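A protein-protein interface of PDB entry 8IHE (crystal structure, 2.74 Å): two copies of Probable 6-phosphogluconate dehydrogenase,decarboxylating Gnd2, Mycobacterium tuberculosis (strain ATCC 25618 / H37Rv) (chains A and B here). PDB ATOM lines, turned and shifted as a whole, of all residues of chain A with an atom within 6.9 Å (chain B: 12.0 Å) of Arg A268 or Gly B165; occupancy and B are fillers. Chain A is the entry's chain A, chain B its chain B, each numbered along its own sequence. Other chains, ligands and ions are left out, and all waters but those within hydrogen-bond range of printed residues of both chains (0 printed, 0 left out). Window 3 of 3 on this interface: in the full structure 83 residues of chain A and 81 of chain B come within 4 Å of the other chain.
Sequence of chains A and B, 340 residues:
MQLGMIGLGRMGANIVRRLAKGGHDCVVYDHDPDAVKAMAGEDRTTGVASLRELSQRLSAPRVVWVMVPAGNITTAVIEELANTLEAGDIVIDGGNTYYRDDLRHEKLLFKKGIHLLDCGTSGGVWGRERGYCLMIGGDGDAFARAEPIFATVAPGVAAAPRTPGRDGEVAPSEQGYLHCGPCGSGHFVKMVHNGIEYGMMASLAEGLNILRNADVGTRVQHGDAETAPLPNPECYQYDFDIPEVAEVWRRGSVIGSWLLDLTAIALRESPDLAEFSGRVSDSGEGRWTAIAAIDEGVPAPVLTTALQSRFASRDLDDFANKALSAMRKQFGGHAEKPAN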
ATOM      1  N   PRO A 243      -3.693 -28.863 -14.257  1.00  0.00           N
ATOM      2  CA  PRO A 243      -2.900 -27.726 -14.730  1.00  0.00           C
ATOM      3  C   PRO A 243      -1.473 -28.123 -15.133  1.00  0.00           C
ATOM      4  O   PRO A 243      -0.949 -27.514 -16.051  1.00  0.00           O
ATOM      5  CB  PRO A 243      -2.873 -26.762 -13.550  1.00  0.00           C
ATOM      6  CG  PRO A 243      -4.094 -27.149 -12.732  1.00  0.00           C
ATOM      7  CD  PRO A 243      -4.241 -28.642 -12.907  1.00  0.00           C
ATOM      8  N   GLU A 244      -0.881 -29.110 -14.455  1.00  0.00           N
ATOM      9  CA  GLU A 244       0.524 -29.521 -14.710  1.00  0.00           C
ATOM     10  C   GLU A 244       0.572 -30.504 -15.880  1.00  0.00           C
ATOM     11  O   GLU A 244       1.587 -30.428 -16.628  1.00  0.00           O
ATOM     12  CB  GLU A 244       1.182 -30.087 -13.446  1.00  0.00           C
ATOM     13  CG  GLU A 244       1.367 -29.052 -12.353  1.00  0.00           C
ATOM     14  CD  GLU A 244       2.317 -27.922 -12.720  1.00  0.00           C
ATOM     15  OE1 GLU A 244       3.244 -27.640 -11.940  1.00  0.00           O
ATOM     16  OE2 GLU A 244       2.127 -27.309 -13.774  1.00  0.00           O
ATOM     17  N   GLU A 247       0.114 -28.564 -19.009  1.00  0.00           N
ATOM     18  CA  GLU A 247       1.433 -27.908 -19.258  1.00  0.00           C
ATOM     19  C   GLU A 247       2.457 -28.921 -19.807  1.00  0.00           C
ATOM     20  O   GLU A 247       3.204 -28.516 -20.718  1.00  0.00           O
ATOM     21  CB  GLU A 247       1.988 -27.276 -17.983  1.00  0.00           C
ATOM     22  CG  GLU A 247       3.353 -26.641 -18.164  1.00  0.00           C
ATOM     23  CD  GLU A 247       3.315 -25.381 -19.007  1.00  0.00           C
ATOM     24  OE1 GLU A 247       4.240 -25.217 -19.857  1.00  0.00           O
ATOM     25  OE2 GLU A 247       2.359 -24.545 -18.800  1.00  0.00           O
ATOM     26  N   LEU A 262      -3.516 -22.379 -24.669  1.00  0.00           N
ATOM     27  CA  LEU A 262      -4.583 -21.550 -24.020  1.00  0.00           C
ATOM     28  C   LEU A 262      -5.137 -22.264 -22.784  1.00  0.00           C
ATOM     29  O   LEU A 262      -5.245 -21.597 -21.694  1.00  0.00           O
ATOM     30  CB  LEU A 262      -5.738 -21.273 -24.982  1.00  0.00           C
ATOM     31  CG  LEU A 262      -5.392 -20.405 -26.184  1.00  0.00           C
ATOM     32  CD1 LEU A 262      -6.632 -20.116 -27.007  1.00  0.00           C
ATOM     33  CD2 LEU A 262      -4.735 -19.112 -25.755  1.00  0.00           C
ATOM     34  N   THR A 263      -5.499 -23.548 -22.945  1.00  0.00           N
ATOM     35  CA  THR A 263      -6.030 -24.421 -21.872  1.00  0.00           C
ATOM     36  C   THR A 263      -5.047 -24.446 -20.692  1.00  0.00           C
ATOM     37  O   THR A 263      -5.517 -24.396 -19.541  1.00  0.00           O
ATOM     38  CB  THR A 263      -6.277 -25.822 -22.420  1.00  0.00           C
ATOM     39  OG1 THR A 263      -7.181 -25.668 -23.512  1.00  0.00           O
ATOM     40  CG2 THR A 263      -6.865 -26.765 -21.392  1.00  0.00           C
ATOM     41  N   ALA A 264      -3.731 -24.506 -20.964  1.00  0.00           N
ATOM     42  CA  ALA A 264      -2.655 -24.478 -19.935  1.00  0.00           C
ATOM     43  C   ALA A 264      -2.784 -23.183 -19.129  1.00  0.00           C
ATOM     44  O   ALA A 264      -2.938 -23.261 -17.918  1.00  0.00           O
ATOM     45  CB  ALA A 264      -1.287 -24.591 -20.563  1.00  0.00           C
ATOM     46  N   ILE A 265      -2.775 -22.035 -19.807  1.00  0.00           N
ATOM     47  CA  ILE A 265      -2.935 -20.692 -19.171  1.00  0.00           C
ATOM     48  C   ILE A 265      -4.208 -20.697 -18.313  1.00  0.00           C
ATOM     49  O   ILE A 265      -4.119 -20.327 -17.107  1.00  0.00           O
ATOM     50  CB  ILE A 265      -2.964 -19.581 -20.238  1.00  0.00           C
ATOM     51  CG1 ILE A 265      -1.693 -19.594 -21.092  1.00  0.00           C
ATOM     52  CG2 ILE A 265      -3.204 -18.221 -19.599  1.00  0.00           C
ATOM     53  CD1 ILE A 265      -1.668 -18.565 -22.208  1.00  0.00           C
ATOM     54  N   ALA A 266      -5.349 -21.106 -18.901  1.00  0.00           N
ATOM     55  CA  ALA A 266      -6.673 -21.075 -18.232  1.00  0.00           C
ATOM     56  C   ALA A 266      -6.617 -21.882 -16.933  1.00  0.00           C
ATOM     57  O   ALA A 266      -7.068 -21.365 -15.919  1.00  0.00           O
ATOM     58  CB  ALA A 266      -7.729 -21.583 -19.151  1.00  0.00           C
ATOM     59  N   LEU A 267      -6.017 -23.068 -16.961  1.00  0.00           N
ATOM     60  CA  LEU A 267      -5.882 -23.981 -15.793  1.00  0.00           C
ATOM     61  C   LEU A 267      -4.842 -23.440 -14.787  1.00  0.00           C
ATOM     62  O   LEU A 267      -4.938 -23.777 -13.558  1.00  0.00           O
ATOM     63  CB  LEU A 267      -5.491 -25.370 -16.318  1.00  0.00           C
ATOM     64  CG  LEU A 267      -6.626 -26.191 -16.939  1.00  0.00           C
ATOM     65  CD1 LEU A 267      -6.095 -27.433 -17.632  1.00  0.00           C
ATOM     66  CD2 LEU A 267      -7.651 -26.585 -15.890  1.00  0.00           C
ATOM     67  N   ARG A 268      -3.858 -22.668 -15.265  1.00  0.00           N
ATOM     68  CA  ARG A 268      -2.836 -22.012 -14.409  1.00  0.00           C
ATOM     69  C   ARG A 268      -3.565 -20.958 -13.560  1.00  0.00           C
ATOM     70  O   ARG A 268      -3.556 -21.117 -12.311  1.00  0.00           O
ATOM     71  CB  ARG A 268      -1.720 -21.471 -15.305  1.00  0.00           C
ATOM     72  CG  ARG A 268      -0.588 -20.759 -14.587  1.00  0.00           C
ATOM     73  CD  ARG A 268       0.268 -21.661 -13.733  1.00  0.00           C
ATOM     74  NE  ARG A 268       1.396 -20.896 -13.229  1.00  0.00           N
ATOM     75  CZ  ARG A 268       2.377 -21.391 -12.478  1.00  0.00           C
ATOM     76  NH1 ARG A 268       2.382 -22.675 -12.156  1.00  0.00           N
ATOM     77  NH2 ARG A 268       3.353 -20.593 -12.057  1.00  0.00           N
ATOM     78  N   GLU A 269      -4.283 -20.021 -14.210  1.00  0.00           N
ATOM     79  CA  GLU A 269      -5.125 -18.964 -13.560  1.00  0.00           C
ATOM     80  C   GLU A 269      -6.187 -19.581 -12.630  1.00  0.00           C
ATOM     81  O   GLU A 269      -6.598 -18.895 -11.669  1.00  0.00           O
ATOM     82  CB  GLU A 269      -5.889 -18.095 -14.568  1.00  0.00           C
ATOM     83  CG  GLU A 269      -5.029 -17.340 -15.568  1.00  0.00           C
ATOM     84  CD  GLU A 269      -5.802 -16.594 -16.654  1.00  0.00           C
ATOM     85  OE1 GLU A 269      -5.142 -15.867 -17.450  1.00  0.00           O
ATOM     86  OE2 GLU A 269      -7.064 -16.715 -16.702  1.00  0.00           O
ATOM     87  N   SER A 270      -6.668 -20.792 -12.930  1.00  0.00           N
ATOM     88  CA  SER A 270      -7.939 -21.334 -12.384  1.00  0.00           C
ATOM     89  C   SER A 270      -8.001 -22.858 -12.479  1.00  0.00           C
ATOM     90  O   SER A 270      -8.668 -23.409 -13.343  1.00  0.00           O
ATOM     91  CB  SER A 270      -9.104 -20.722 -13.091  1.00  0.00           C
ATOM     92  OG  SER A 270     -10.277 -21.459 -12.779  1.00  0.00           O
ATOM     93  N   PRO A 271      -7.384 -23.593 -11.539  1.00  0.00           N
ATOM     94  CA  PRO A 271      -7.229 -25.045 -11.680  1.00  0.00           C
ATOM     95  C   PRO A 271      -8.454 -25.964 -11.485  1.00  0.00           C
ATOM     96  O   PRO A 271      -8.289 -27.136 -11.648  1.00  0.00           O
ATOM     97  CB  PRO A 271      -6.206 -25.359 -10.574  1.00  0.00           C
ATOM     98  CG  PRO A 271      -5.562 -24.016 -10.266  1.00  0.00           C
ATOM     99  CD  PRO A 271      -6.723 -23.054 -10.347  1.00  0.00           C
ATOM    100  N   VAL B 157      12.453 -27.023 -21.367  1.00  0.00           N
ATOM    101  CA  VAL B 157      11.582 -25.806 -21.381  1.00  0.00           C
ATOM    102  C   VAL B 157      11.741 -25.067 -22.709  1.00  0.00           C
ATOM    103  O   VAL B 157      10.747 -24.534 -23.218  1.00  0.00           O
ATOM    104  CB  VAL B 157      11.905 -24.856 -20.205  1.00  0.00           C
ATOM    105  CG1 VAL B 157      13.023 -23.866 -20.541  1.00  0.00           C
ATOM    106  CG2 VAL B 157      10.665 -24.101 -19.730  1.00  0.00           C
ATOM    107  N   ALA B 160       9.493 -24.459 -26.145  1.00  0.00           N
ATOM    108  CA  ALA B 160       8.291 -23.608 -26.311  1.00  0.00           C
ATOM    109  C   ALA B 160       8.228 -22.492 -25.272  1.00  0.00           C
ATOM    110  O   ALA B 160       8.374 -22.717 -24.070  1.00  0.00           O
ATOM    111  CB  ALA B 160       7.052 -24.471 -26.225  1.00  0.00           C
ATOM    112  N   PRO B 161       7.900 -21.263 -25.703  1.00  0.00           N
ATOM    113  CA  PRO B 161       7.793 -20.123 -24.794  1.00  0.00           C
ATOM    114  C   PRO B 161       7.070 -20.464 -23.488  1.00  0.00           C
ATOM    115  O   PRO B 161       6.095 -21.165 -23.557  1.00  0.00           O
ATOM    116  CB  PRO B 161       6.966 -19.137 -25.621  1.00  0.00           C
ATOM    117  CG  PRO B 161       7.399 -19.409 -27.049  1.00  0.00           C
ATOM    118  CD  PRO B 161       7.620 -20.907 -27.095  1.00  0.00           C
ATOM    119  N   ARG B 162       7.550 -19.979 -22.343  1.00  0.00           N
ATOM    120  CA  ARG B 162       7.002 -20.374 -21.015  1.00  0.00           C
ATOM    121  C   ARG B 162       5.532 -19.948 -20.970  1.00  0.00           C
ATOM    122  O   ARG B 162       5.209 -18.977 -21.631  1.00  0.00           O
ATOM    123  CB  ARG B 162       7.847 -19.756 -19.896  1.00  0.00           C
ATOM    124  CG  ARG B 162       9.219 -20.399 -19.738  1.00  0.00           C
ATOM    125  CD  ARG B 162       9.864 -20.179 -18.383  1.00  0.00           C
ATOM    126  NE  ARG B 162       9.039 -20.547 -17.224  1.00  0.00           N
ATOM    127  CZ  ARG B 162       9.457 -20.539 -15.949  1.00  0.00           C
ATOM    128  NH1 ARG B 162      10.706 -20.210 -15.648  1.00  0.00           N
ATOM    129  NH2 ARG B 162       8.626 -20.867 -14.972  1.00  0.00           N
ATOM    130  N   THR B 163       4.659 -20.684 -20.282  1.00  0.00           N
ATOM    131  CA  THR B 163       3.226 -20.301 -20.099  1.00  0.00           C
ATOM    132  C   THR B 163       3.205 -18.907 -19.478  1.00  0.00           C
ATOM    133  O   THR B 163       3.933 -18.651 -18.526  1.00  0.00           O
ATOM    134  CB  THR B 163       2.462 -21.359 -19.276  1.00  0.00           C
ATOM    135  OG1 THR B 163       1.962 -22.408 -20.109  1.00  0.00           O
ATOM    136  CG2 THR B 163       1.273 -20.814 -18.531  1.00  0.00           C
ATOM    137  N   PRO B 164       2.441 -17.933 -20.021  1.00  0.00           N
ATOM    138  CA  PRO B 164       2.169 -16.681 -19.311  1.00  0.00           C
ATOM    139  C   PRO B 164       1.622 -16.911 -17.897  1.00  0.00           C
ATOM    140  O   PRO B 164       0.577 -17.506 -17.755  1.00  0.00           O
ATOM    141  CB  PRO B 164       1.123 -15.984 -20.189  1.00  0.00           C
ATOM    142  CG  PRO B 164       1.424 -16.498 -21.588  1.00  0.00           C
ATOM    143  CD  PRO B 164       1.874 -17.937 -21.380  1.00  0.00           C
ATOM    144  N   GLY B 165       2.356 -16.433 -16.890  1.00  0.00           N
ATOM    145  CA  GLY B 165       2.011 -16.622 -15.471  1.00  0.00           C
ATOM    146  C   GLY B 165       2.988 -17.565 -14.802  1.00  0.00           C
ATOM    147  O   GLY B 165       3.083 -17.537 -13.557  1.00  0.00           O
ATOM    148  N   ARG B 166       3.672 -18.394 -15.594  1.00  0.00           N
ATOM    149  CA  ARG B 166       4.817 -19.200 -15.110  1.00  0.00           C
ATOM    150  C   ARG B 166       5.920 -18.210 -14.767  1.00  0.00           C
ATOM    151  O   ARG B 166       6.586 -17.752 -15.694  1.00  0.00           O
ATOM    152  CB  ARG B 166       5.289 -20.224 -16.143  1.00  0.00           C
ATOM    153  CG  ARG B 166       4.382 -21.436 -16.268  1.00  0.00           C
ATOM    154  CD  ARG B 166       4.478 -22.416 -15.119  1.00  0.00           C
ATOM    155  NE  ARG B 166       3.295 -23.237 -15.168  1.00  0.00           N
ATOM    156  CZ  ARG B 166       3.221 -24.511 -14.826  1.00  0.00           C
ATOM    157  NH1 ARG B 166       4.287 -25.147 -14.365  1.00  0.00           N
ATOM    158  NH2 ARG B 166       2.060 -25.143 -14.930  1.00  0.00           N
ATOM    159  N   ASP B 167       5.995 -17.846 -13.487  1.00  0.00           N
ATOM    160  CA  ASP B 167       7.053 -16.994 -12.888  1.00  0.00           C
ATOM    161  C   ASP B 167       8.174 -17.921 -12.393  1.00  0.00           C
ATOM    162  O   ASP B 167       7.950 -19.149 -12.347  1.00  0.00           O
ATOM    163  CB  ASP B 167       6.490 -16.120 -11.753  1.00  0.00           C
ATOM    164  CG  ASP B 167       5.392 -15.138 -12.150  1.00  0.00           C
ATOM    165  OD1 ASP B 167       5.185 -14.926 -13.370  1.00  0.00           O
ATOM    166  OD2 ASP B 167       4.748 -14.585 -11.230  1.00  0.00           O
ATOM    167  N   GLY B 168       9.337 -17.348 -12.074  1.00  0.00           N
ATOM    168  CA  GLY B 168      10.375 -17.963 -11.223  1.00  0.00           C
ATOM    169  C   GLY B 168      11.056 -19.147 -11.887  1.00  0.00           C
ATOM    170  O   GLY B 168      11.592 -18.960 -12.994  1.00  0.00           O
ATOM    171  N   GLU B 169      11.038 -20.314 -11.224  1.00  0.00           N
ATOM    172  CA  GLU B 169      11.838 -21.516 -11.595  1.00  0.00           C
ATOM    173  C   GLU B 169      11.013 -22.436 -12.506  1.00  0.00           C
ATOM    174  O   GLU B 169       9.822 -22.696 -12.205  1.00  0.00           O
ATOM    175  CB  GLU B 169      12.341 -22.288 -10.367  1.00  0.00           C
ATOM    176  CG  GLU B 169      13.657 -21.761  -9.790  1.00  0.00           C
ATOM    177  CD  GLU B 169      14.727 -22.795  -9.435  1.00  0.00           C
ATOM    178  OE1 GLU B 169      14.383 -23.886  -8.915  1.00  0.00           O
ATOM    179  OE2 GLU B 169      15.920 -22.508  -9.692  1.00  0.00           O
ATOM    180  N   VAL B 170      11.668 -22.884 -13.581  1.00  0.00           N
ATOM    181  CA  VAL B 170      11.194 -23.876 -14.587  1.00  0.00           C
ATOM    182  C   VAL B 170      10.872 -25.170 -13.851  1.00  0.00           C
ATOM    183  O   VAL B 170      11.835 -25.828 -13.419  1.00  0.00           O
ATOM    184  CB  VAL B 170      12.284 -24.130 -15.647  1.00  0.00           C
ATOM    185  CG1 VAL B 170      11.977 -25.360 -16.482  1.00  0.00           C
ATOM    186  CG2 VAL B 170      12.521 -22.921 -16.544  1.00  0.00           C
ATOM    187  N   ALA B 171       9.588 -25.541 -13.770  1.00  0.00           N
ATOM    188  CA  ALA B 171       9.076 -26.776 -13.107  1.00  0.00           C
ATOM    189  C   ALA B 171       9.351 -28.031 -13.950  1.00  0.00           C
ATOM    190  O   ALA B 171       9.740 -27.958 -15.124  1.00  0.00           O
ATOM    191  CB  ALA B 171       7.602 -26.611 -12.827  1.00  0.00           C
ATOM    192  N   PRO B 172       9.157 -29.249 -13.392  1.00  0.00           N
ATOM    193  CA  PRO B 172       9.307 -30.464 -14.194  1.00  0.00           C
ATOM    194  C   PRO B 172       8.366 -30.418 -15.422  1.00  0.00           C
ATOM    195  O   PRO B 172       8.843 -30.514 -16.549  1.00  0.00           O
ATOM    196  CB  PRO B 172       8.952 -31.601 -13.216  1.00  0.00           C
ATOM    197  CG  PRO B 172       9.016 -30.980 -11.827  1.00  0.00           C
ATOM    198  CD  PRO B 172       8.717 -29.514 -12.009  1.00  0.00           C
ATOM    199  N   SER B 173       7.060 -30.235 -15.185  1.00  0.00           N
ATOM    200  CA  SER B 173       6.004 -30.017 -16.210  1.00  0.00           C
ATOM    201  C   SER B 173       6.543 -29.271 -17.426  1.00  0.00           C
ATOM    202  O   SER B 173       6.269 -29.717 -18.545  1.00  0.00           O
ATOM    203  CB  SER B 173       4.836 -29.239 -15.630  1.00  0.00           C
ATOM    204  OG  SER B 173       5.108 -27.846 -15.605  1.00  0.00           O
ATOM    205  N   GLU B 174       7.211 -28.141 -17.205  1.00  0.00           N
ATOM    206  CA  GLU B 174       7.577 -27.177 -18.276  1.00  0.00           C
ATOM    207  C   GLU B 174       8.747 -27.715 -19.111  1.00  0.00           C
ATOM    208  O   GLU B 174       8.940 -27.214 -20.252  1.00  0.00           O
ATOM    209  CB  GLU B 174       8.010 -25.824 -17.700  1.00  0.00           C
ATOM    210  CG  GLU B 174       7.018 -25.170 -16.765  1.00  0.00           C
ATOM    211  CD  GLU B 174       7.444 -23.793 -16.280  1.00  0.00           C
ATOM    212  OE1 GLU B 174       7.579 -22.893 -17.139  1.00  0.00           O
ATOM    213  OE2 GLU B 174       7.623 -23.617 -15.038  1.00  0.00           O
ATOM    214  N   GLN B 175       9.525 -28.644 -18.533  1.00  0.00           N
ATOM    215  CA  GLN B 175      10.728 -29.263 -19.144  1.00  0.00           C
ATOM    216  C   GLN B 175      10.317 -30.368 -20.122  1.00  0.00           C
ATOM    217  O   GLN B 175      11.182 -30.804 -20.918  1.00  0.00           O
ATOM    218  CB  GLN B 175      11.629 -29.858 -18.058  1.00  0.00           C
ATOM    219  CG  GLN B 175      12.095 -28.853 -17.002  1.00  0.00           C
ATOM    220  CD  GLN B 175      13.337 -28.055 -17.341  1.00  0.00           C
ATOM    221  OE1 GLN B 175      13.631 -27.714 -18.487  1.00  0.00           O
ATOM    222  NE2 GLN B 175      14.059 -27.673 -16.305  1.00  0.00           N
ATOM    223  N   LEU B 178       6.887 -35.082 -16.168  1.00  0.00           N
ATOM    224  CA  LEU B 178       6.122 -34.859 -14.929  1.00  0.00           C
ATOM    225  C   LEU B 178       5.844 -36.186 -14.239  1.00  0.00           C
ATOM    226  O   LEU B 178       5.636 -37.213 -14.938  1.00  0.00           O
ATOM    227  CB  LEU B 178       4.807 -34.166 -15.262  1.00  0.00           C
ATOM    228  CG  LEU B 178       3.826 -34.037 -14.097  1.00  0.00           C
ATOM    229  CD1 LEU B 178       3.877 -32.628 -13.518  1.00  0.00           C
ATOM    230  CD2 LEU B 178       2.410 -34.369 -14.551  1.00  0.00           C
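The side-chain hydroxyl (OG) of Ser B173 is in hydrogen-bond range of the guanidinium group (NH1) of Arg B166, 3.1 Å away. OE2 of Glu B174 lies within salt-bridge range of NH1 of Arg B166, at 3.7 Å.
Gly B165 touches one residue of chain A. Ile A265 touches just one residue of chain B: Pro B164 (3.7 Å). No residue of chain B comes within 4 Å of Ala A266. No residue of chain B comes within 4 Å of Ser A270. No residue of chain B comes within 4 Å of Pro A271. Printed residues of chain A within 4 Å of Ser B173: Glu A244 and Glu A247. Printed residues of chain A within 4 Å of Arg B166: Pro A243 (3.99 Å), Glu A244 (2.5 Å), Glu A247 (3.7 Å) and Arg A268 (3.2 Å). Of the printed residues of chain A, Pro B164 touches Ile A265 (3.7 Å). Val B170 touches none of the printed residues of chain A.
No position is printed for both chains.
The side-chain carboxylate (OE2) of Glu A244 is in salt-bridge range of the guanidinium group (NH2) of Arg B166 (2.5 Å). The side-chain hydroxyl of Thr B163 sits at hydrogen-bond distance from the side-chain carboxylate of Glu A247 (2.5 Å). NH2 of Arg B166 lies within salt-bridge range of OE2 of Glu A247 (3.9 Å). NH2 of Arg A268 lies within hydrogen-bond range of O of Gly B165, 3.4 Å away. The guanidinium group of Arg B166 sits close to the guanidinium group of Arg A268 (3.2 Å).
Of the 18 printed residues of chain B, 6 touch a printed residue of chain A. Hydrophobic or aromatic side chains of chain B within 4 Å of the printed part of chain A: Pro B164 and Leu B178.
Among the printed residues, pairs that only touch across the chains: Glu A247 with Ser B173 (3.3 Å), Glu A244 with Ser B173 (3.5 Å), Ile A265 with Pro B164 (3.7 Å), Glu A244 with Leu B178 (3.7 Å), Ala A264 with Thr B163 (3.9 Å) and Pro A243 with Arg B166 (3.99 Å).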
